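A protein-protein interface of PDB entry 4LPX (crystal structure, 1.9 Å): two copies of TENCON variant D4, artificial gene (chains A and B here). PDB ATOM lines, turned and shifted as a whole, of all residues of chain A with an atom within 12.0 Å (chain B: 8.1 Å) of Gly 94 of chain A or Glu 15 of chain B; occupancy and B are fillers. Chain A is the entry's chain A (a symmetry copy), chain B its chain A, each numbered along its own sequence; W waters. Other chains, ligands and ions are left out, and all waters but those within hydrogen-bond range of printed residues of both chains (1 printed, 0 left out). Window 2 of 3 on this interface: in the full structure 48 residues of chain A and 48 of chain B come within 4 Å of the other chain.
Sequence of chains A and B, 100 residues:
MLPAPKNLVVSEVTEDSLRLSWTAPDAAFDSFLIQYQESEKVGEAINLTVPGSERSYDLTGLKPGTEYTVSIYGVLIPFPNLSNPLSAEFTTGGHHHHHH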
ATOM      1  N   PHE A  90      -2.632 -13.836 -36.296  1.00  0.00           N
ATOM      2  CA  PHE A  90      -3.313 -14.117 -35.041  1.00  0.00           C
ATOM      3  C   PHE A  90      -3.879 -12.826 -34.447  1.00  0.00           C
ATOM      4  O   PHE A  90      -3.324 -11.739 -34.663  1.00  0.00           O
ATOM      5  CB  PHE A  90      -2.373 -14.774 -34.016  1.00  0.00           C
ATOM      6  CG  PHE A  90      -1.830 -16.120 -34.437  1.00  0.00           C
ATOM      7  CD1 PHE A  90      -2.681 -17.121 -34.931  1.00  0.00           C
ATOM      8  CD2 PHE A  90      -0.458 -16.389 -34.336  1.00  0.00           C
ATOM      9  CE1 PHE A  90      -2.189 -18.361 -35.319  1.00  0.00           C
ATOM     10  CE2 PHE A  90       0.048 -17.639 -34.724  1.00  0.00           C
ATOM     11  CZ  PHE A  90      -0.816 -18.627 -35.215  1.00  0.00           C
ATOM     12  N   THR A  91      -4.975 -12.954 -33.704  1.00  0.00           N
ATOM     13  CA  THR A  91      -5.757 -11.790 -33.269  1.00  0.00           C
ATOM     14  C   THR A  91      -5.952 -11.858 -31.757  1.00  0.00           C
ATOM     15  O   THR A  91      -6.413 -12.873 -31.221  1.00  0.00           O
ATOM     16  CB  THR A  91      -7.147 -11.731 -34.004  1.00  0.00           C
ATOM     17  OG1 THR A  91      -6.947 -11.763 -35.419  1.00  0.00           O
ATOM     18  CG2 THR A  91      -7.937 -10.446 -33.647  1.00  0.00           C
ATOM     19  N   THR A  92      -5.601 -10.770 -31.065  1.00  0.00           N
ATOM     20  CA  THR A  92      -5.781 -10.720 -29.623  1.00  0.00           C
ATOM     21  C   THR A  92      -7.280 -10.586 -29.300  1.00  0.00           C
ATOM     22  O   THR A  92      -8.047 -10.111 -30.136  1.00  0.00           O
ATOM     23  CB  THR A  92      -5.040  -9.507 -29.008  1.00  0.00           C
ATOM     24  OG1 THR A  92      -5.365  -8.339 -29.760  1.00  0.00           O
ATOM     25  CG2 THR A  92      -3.514  -9.723 -29.032  1.00  0.00           C
ATOM     26  N   GLY A  93      -7.673 -11.004 -28.101  1.00  0.00           N
ATOM     27  CA  GLY A  93      -9.055 -10.841 -27.617  1.00  0.00           C
ATOM     28  C   GLY A  93      -9.483  -9.391 -27.418  1.00  0.00           C
ATOM     29  O   GLY A  93      -8.666  -8.462 -27.512  1.00  0.00           O
ATOM     30  N   GLY A  94     -10.774  -9.197 -27.144  1.00  0.00           N
ATOM     31  CA  GLY A  94     -11.333  -7.863 -26.895  1.00  0.00           C
ATOM     32  C   GLY A  94     -11.662  -7.084 -28.159  1.00  0.00           C
ATOM     33  O   GLY A  94     -11.700  -7.648 -29.253  1.00  0.00           O
ATOM     34  N   HIS A  95     -11.900  -5.779 -28.003  1.00  0.00           N
ATOM     35  CA  HIS A  95     -12.248  -4.900 -29.125  1.00  0.00           C
ATOM     36  C   HIS A  95     -11.209  -3.787 -29.306  1.00  0.00           C
ATOM     37  O   HIS A  95     -10.614  -3.326 -28.330  1.00  0.00           O
ATOM     38  CB  HIS A  95     -13.654  -4.307 -28.922  1.00  0.00           C
ATOM     39  N   HIS A  96     -10.997  -3.364 -30.553  1.00  0.00           N
ATOM     40  CA  HIS A  96     -10.048  -2.286 -30.871  1.00  0.00           C
ATOM     41  C   HIS A  96     -10.600  -0.912 -30.482  1.00  0.00           C
ATOM     42  O   HIS A  96     -11.726  -0.566 -30.850  1.00  0.00           O
ATOM     43  CB  HIS A  96      -9.676  -2.318 -32.361  1.00  0.00           C
ATOM     44  N   HIS A  97      -9.806  -0.135 -29.739  1.00  0.00           N
ATOM     45  CA  HIS A  97     -10.220   1.196 -29.269  1.00  0.00           C
ATOM     46  C   HIS A  97      -9.308   2.307 -29.788  1.00  0.00           C
ATOM     47  O   HIS A  97      -9.052   2.399 -31.003  1.00  0.00           O
ATOM     48  CB  HIS A  97     -10.284   1.231 -27.743  1.00  0.00           C
ATOM     49  N   GLU B  12      -3.607 -19.354 -25.399  1.00  0.00           N
ATOM     50  CA  GLU B  12      -3.568 -18.337 -24.337  1.00  0.00           C
ATOM     51  C   GLU B  12      -3.767 -16.928 -24.892  1.00  0.00           C
ATOM     52  O   GLU B  12      -3.012 -15.995 -24.604  1.00  0.00           O
ATOM     53  CB  GLU B  12      -2.259 -18.453 -23.535  1.00  0.00           C
ATOM     54  CG  GLU B  12      -1.971 -19.893 -23.077  1.00  0.00           C
ATOM     55  CD  GLU B  12      -0.839 -19.999 -22.066  1.00  0.00           C
ATOM     56  OE1 GLU B  12      -0.572 -21.133 -21.610  1.00  0.00           O
ATOM     57  OE2 GLU B  12      -0.218 -18.965 -21.726  1.00  0.00           O
ATOM     58  N   VAL B  13      -4.808 -16.785 -25.704  1.00  0.00           N
ATOM     59  CA  VAL B  13      -5.113 -15.517 -26.332  1.00  0.00           C
ATOM     60  C   VAL B  13      -5.737 -14.598 -25.281  1.00  0.00           C
ATOM     61  O   VAL B  13      -6.761 -14.936 -24.699  1.00  0.00           O
ATOM     62  CB  VAL B  13      -6.091 -15.720 -27.507  1.00  0.00           C
ATOM     63  CG1 VAL B  13      -6.458 -14.378 -28.149  1.00  0.00           C
ATOM     64  CG2 VAL B  13      -5.494 -16.717 -28.540  1.00  0.00           C
ATOM     65  N   THR B  14      -5.116 -13.444 -25.044  1.00  0.00           N
ATOM     66  CA  THR B  14      -5.667 -12.444 -24.131  1.00  0.00           C
ATOM     67  C   THR B  14      -5.832 -11.144 -24.909  1.00  0.00           C
ATOM     68  O   THR B  14      -5.658 -11.109 -26.134  1.00  0.00           O
ATOM     69  CB  THR B  14      -4.756 -12.210 -22.872  1.00  0.00           C
ATOM     70  OG1 THR B  14      -3.593 -11.460 -23.250  1.00  0.00           O
ATOM     71  CG2 THR B  14      -4.346 -13.524 -22.214  1.00  0.00           C
ATOM     72  N   GLU B  15      -6.168 -10.067 -24.206  1.00  0.00           N
ATOM     73  CA  GLU B  15      -6.271  -8.756 -24.838  1.00  0.00           C
ATOM     74  C   GLU B  15      -4.915  -8.134 -25.174  1.00  0.00           C
ATOM     75  O   GLU B  15      -4.831  -7.228 -25.998  1.00  0.00           O
ATOM     76  CB  GLU B  15      -7.083  -7.798 -23.954  1.00  0.00           C
ATOM     77  CG  GLU B  15      -8.461  -8.337 -23.589  1.00  0.00           C
ATOM     78  CD  GLU B  15      -9.485  -7.236 -23.357  1.00  0.00           C
ATOM     79  OE1 GLU B  15      -9.098  -6.075 -23.107  1.00  0.00           O
ATOM     80  OE2 GLU B  15     -10.690  -7.538 -23.428  1.00  0.00           O
ATOM     81  N   ASP B  16      -3.852  -8.621 -24.539  1.00  0.00           N
ATOM     82  CA  ASP B  16      -2.529  -8.004 -24.693  1.00  0.00           C
ATOM     83  C   ASP B  16      -1.389  -9.002 -24.924  1.00  0.00           C
ATOM     84  O   ASP B  16      -0.220  -8.607 -24.940  1.00  0.00           O
ATOM     85  CB  ASP B  16      -2.210  -7.123 -23.471  1.00  0.00           C
ATOM     86  CG  ASP B  16      -2.468  -7.837 -22.148  1.00  0.00           C
ATOM     87  OD1 ASP B  16      -1.886  -8.921 -21.913  1.00  0.00           O
ATOM     88  OD2 ASP B  16      -3.258  -7.310 -21.338  1.00  0.00           O
ATOM     89  N   SER B  17      -1.730 -10.278 -25.102  1.00  0.00           N
ATOM     90  CA  SER B  17      -0.732 -11.338 -25.230  1.00  0.00           C
ATOM     91  C   SER B  17      -1.244 -12.536 -26.041  1.00  0.00           C
ATOM     92  O   SER B  17      -2.454 -12.783 -26.113  1.00  0.00           O
ATOM     93  CB  SER B  17      -0.232 -11.788 -23.844  1.00  0.00           C
ATOM     94  OG  SER B  17      -1.216 -12.535 -23.146  1.00  0.00           O
ATOM     95  N   LEU B  18      -0.303 -13.263 -26.643  1.00  0.00           N
ATOM     96  CA  LEU B  18      -0.575 -14.450 -27.470  1.00  0.00           C
ATOM     97  C   LEU B  18       0.552 -15.458 -27.230  1.00  0.00           C
ATOM     98  O   LEU B  18       1.721 -15.090 -27.326  1.00  0.00           O
ATOM     99  CB  LEU B  18      -0.562 -14.071 -28.958  1.00  0.00           C
ATOM    100  CG  LEU B  18      -1.562 -13.083 -29.561  1.00  0.00           C
ATOM    101  CD1 LEU B  18      -1.172 -12.747 -31.002  1.00  0.00           C
ATOM    102  CD2 LEU B  18      -3.013 -13.609 -29.495  1.00  0.00           C
ATOM    103  N   GLY B  61       2.694  -7.257 -24.517  1.00  0.00           N
ATOM    104  CA  GLY B  61       2.631  -5.830 -24.834  1.00  0.00           C
ATOM    105  C   GLY B  61       1.818  -5.532 -26.085  1.00  0.00           C
ATOM    106  O   GLY B  61       2.098  -4.561 -26.796  1.00  0.00           O
ATOM    107  N   LEU B  62       0.807  -6.362 -26.359  1.00  0.00           N
ATOM    108  CA  LEU B  62      -0.018  -6.190 -27.559  1.00  0.00           C
ATOM    109  C   LEU B  62      -1.285  -5.358 -27.293  1.00  0.00           C
ATOM    110  O   LEU B  62      -1.622  -5.087 -26.137  1.00  0.00           O
ATOM    111  CB  LEU B  62      -0.379  -7.562 -28.163  1.00  0.00           C
ATOM    112  CG  LEU B  62       0.775  -8.545 -28.433  1.00  0.00           C
ATOM    113  CD1 LEU B  62       0.220  -9.869 -28.958  1.00  0.00           C
ATOM    114  CD2 LEU B  62       1.800  -7.975 -29.403  1.00  0.00           C
ATOM    115  N   LYS B  63      -1.965  -4.969 -28.373  1.00  0.00           N
ATOM    116  CA  LYS B  63      -3.208  -4.173 -28.315  1.00  0.00           C
ATOM    117  C   LYS B  63      -4.443  -5.072 -28.448  1.00  0.00           C
ATOM    118  O   LYS B  63      -4.402  -6.053 -29.199  1.00  0.00           O
ATOM    119  CB  LYS B  63      -3.235  -3.157 -29.457  1.00  0.00           C
ATOM    120  CG  LYS B  63      -2.183  -2.064 -29.372  1.00  0.00           C
ATOM    121  CD  LYS B  63      -2.303  -1.119 -30.559  1.00  0.00           C
ATOM    122  CE  LYS B  63      -1.184  -0.088 -30.556  1.00  0.00           C
ATOM    123  NZ  LYS B  63      -1.030   0.532 -31.902  1.00  0.00           N
ATOM    124  N   PRO B  64      -5.544  -4.745 -27.727  1.00  0.00           N
ATOM    125  CA  PRO B  64      -6.771  -5.562 -27.785  1.00  0.00           C
ATOM    126  C   PRO B  64      -7.396  -5.584 -29.180  1.00  0.00           C
ATOM    127  O   PRO B  64      -7.204  -4.645 -29.963  1.00  0.00           O
ATOM    128  CB  PRO B  64      -7.726  -4.874 -26.793  1.00  0.00           C
ATOM    129  CG  PRO B  64      -6.899  -3.910 -26.012  1.00  0.00           C
ATOM    130  CD  PRO B  64      -5.686  -3.584 -26.823  1.00  0.00           C
ATOM    131  N   GLY B  65      -8.138  -6.652 -29.477  1.00  0.00           N
ATOM    132  CA  GLY B  65      -8.819  -6.821 -30.764  1.00  0.00           C
ATOM    133  C   GLY B  65      -8.017  -6.454 -31.999  1.00  0.00           C
ATOM    134  O   GLY B  65      -8.540  -5.798 -32.902  1.00  0.00           O
ATOM    135  N   THR B  66      -6.749  -6.875 -32.041  1.00  0.00           N
ATOM    136  CA  THR B  66      -5.831  -6.474 -33.109  1.00  0.00           C
ATOM    137  C   THR B  66      -5.197  -7.685 -33.793  1.00  0.00           C
ATOM    138  O   THR B  66      -4.755  -8.616 -33.124  1.00  0.00           O
ATOM    139  CB  THR B  66      -4.696  -5.545 -32.566  1.00  0.00           C
ATOM    140  OG1 THR B  66      -5.277  -4.403 -31.920  1.00  0.00           O
ATOM    141  CG2 THR B  66      -3.784  -5.064 -33.693  1.00  0.00           C
ATOM    142  N   TYR B  68      -2.284  -9.556 -35.804  1.00  0.00           N
ATOM    143  CA  TYR B  68      -0.828  -9.531 -35.967  1.00  0.00           C
ATOM    144  C   TYR B  68      -0.390 -10.561 -36.999  1.00  0.00           C
ATOM    145  O   TYR B  68      -0.825 -11.716 -36.955  1.00  0.00           O
ATOM    146  CB  TYR B  68      -0.158  -9.815 -34.619  1.00  0.00           C
ATOM    147  CG  TYR B  68      -0.345  -8.689 -33.639  1.00  0.00           C
ATOM    148  CD1 TYR B  68       0.557  -7.618 -33.606  1.00  0.00           C
ATOM    149  CD2 TYR B  68      -1.423  -8.683 -32.742  1.00  0.00           C
ATOM    150  CE1 TYR B  68       0.395  -6.578 -32.711  1.00  0.00           C
ATOM    151  CE2 TYR B  68      -1.591  -7.631 -31.833  1.00  0.00           C
ATOM    152  CZ  TYR B  68      -0.674  -6.587 -31.829  1.00  0.00           C
ATOM    153  OH  TYR B  68      -0.815  -5.543 -30.949  1.00  0.00           O
HETATM  154  O   HOH W   1      -7.030  -1.793 -29.630  1.00  0.00           O
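No position is printed for both chains.
Gly 93 of chain A touches just these residues of chain B: Val 13 (3.6 Å), Thr 14 (2.8 Å), Glu 15 (3.6 Å), Pro 64 (3.5 Å) and Gly 65 (2.7 Å).
His 95 of chain A touches one residue of chain B.
Thr 14 of chain B touches just these residues of chain A: Thr 92 (3.3 Å) and Gly 93 (2.8 Å).
No residue of chain A comes within 4 Å of Asp 16 of chain B.
Ser 17 of chain B touches none of the printed residues of chain A.
Leu 62 of chain B touches one residue of chain A.
Of chain A, only Thr 92 (3.3 Å), Gly 93 (2.7 Å), Gly 94 (3.4 Å) and His 96 (3.7 Å) come within 4 Å of Gly 65 of chain B.
Of the printed residues of chain B, Thr 91 of chain A touches Val 13 (3.4 Å), Leu 18 (3.9 Å) and Thr 66 (3.3 Å).
Of the printed residues of chain B, Phe 90 of chain A touches Leu 18 (3.8 Å), Thr 66 (3.8 Å) and Tyr 68 (2.7 Å).
Of the printed residues of chain A, Lys 63 of chain B touches Thr 92.
Of the printed residues of chain A, Leu 18 of chain B touches Phe 90 (3.8 Å), Thr 91 (3.9 Å) and Thr 92 (3.9 Å).
Of the printed residues of chain B, His 96 of chain A touches Pro 64 (3.8 Å) and Gly 65 (3.7 Å).
The nearest residue of chain B that does not touch Gly 94 of chain A is Pro 64 of chain B (4.6 Å).
The nearest residue of chain A that does not touch Glu 15 of chain B is His 95 of chain A (5.0 Å).
The nearest printed residue of chain A that does not touch Lys 63 of chain B is Gly 93 of chain A (5.2 Å).
Of the 14 printed residues of chain B, 10 touch a printed residue of chain A.
Hydrophobic or aromatic side chains of chain A within 4 Å of the printed part of chain B: Phe 90 and His 96.
Among the printed residues, 25 pairs touch across the chains.
Among the printed residues, no Asp or Glu carboxylate lies within 4 Å of a Lys or Arg side-chain nitrogen of the other chain.
N of Thr 66 of chain B is in hydrogen-bond range of OG1 of Thr 92 of chain A, at 3.0 Å.
N of Tyr 68 of chain B sits at hydrogen-bond distance from O of Phe 90 of chain A, 2.7 Å away.
N of Gly 65 of chain B sits at hydrogen-bond distance from OG1 of Thr 92 of chain A, 3.3 Å away.
OG1 of Thr 92 of chain A is in hydrogen-bond range of O of Lys 63 of chain B, at 2.5 Å.
The backbone NH (N) of Gly 65 of chain B lies within hydrogen-bond range of the backbone carbonyl oxygen (O) of Gly 93 of chain A (2.7 Å).
The backbone carbonyl oxygen (O) of Thr 14 of chain B sits at hydrogen-bond distance from the backbone NH (N) of Gly 93 of chain A, at 2.8 Å.
Water W1 lies within hydrogen-bond range of O of Pro 64 of chain B and N of His 97 of chain A.
Val 13 of chain B touches Thr 91 of chain A.
O of Thr 66 of chain B touches CA of Thr 91 of chain A, 3.3 Å away.
Thr 92 of chain A touches Leu 18 of chain B (CG2 to CG, 3.9 Å).
Thr 92 of chain A touches Leu 62 of chain B (CG2 to CD1, 3.7 Å).
Tyr 68 of chain B touches Thr 92 of chain A (CE2 to CG2, 3.99 Å).
N of Gly 93 of chain A touches CG1 of Val 13 of chain B (3.6 Å).
Gly 93 of chain A touches Pro 64 of chain B.
Gly 94 of chain A touches Glu 15 of chain B (CA to OE2, 3.5 Å).
CA of His 96 of chain A touches O of Pro 64 of chain B, at 3.8 Å.
Gly 65 of chain B touches His 96 of chain A.
The backbone carbonyl oxygen of Asp 16 of chain B lies within hydrogen-bond range of the backbone NH of Leu 62 of chain B (2.8 Å).
The side-chain hydroxyl of Thr 14 of chain B lies within hydrogen-bond range of the side-chain hydroxyl of Ser 17 of chain B (2.6 Å).
O of Lys 63 of chain B is in hydrogen-bond range of OG1 of Thr 66 of chain B (3.3 Å).
N of Asp 16 of chain B lies within hydrogen-bond range of OG1 of Thr 14 of chain B.
The side-chain hydroxyl of Tyr 68 of chain B lies within hydrogen-bond range of the backbone NH of Lys 63 of chain B (2.9 Å).
The backbone carbonyl oxygen (O) of Pro 64 of chain B lies within hydrogen-bond range of the side-chain hydroxyl (OG1) of Thr 66 of chain B, at 2.8 Å.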
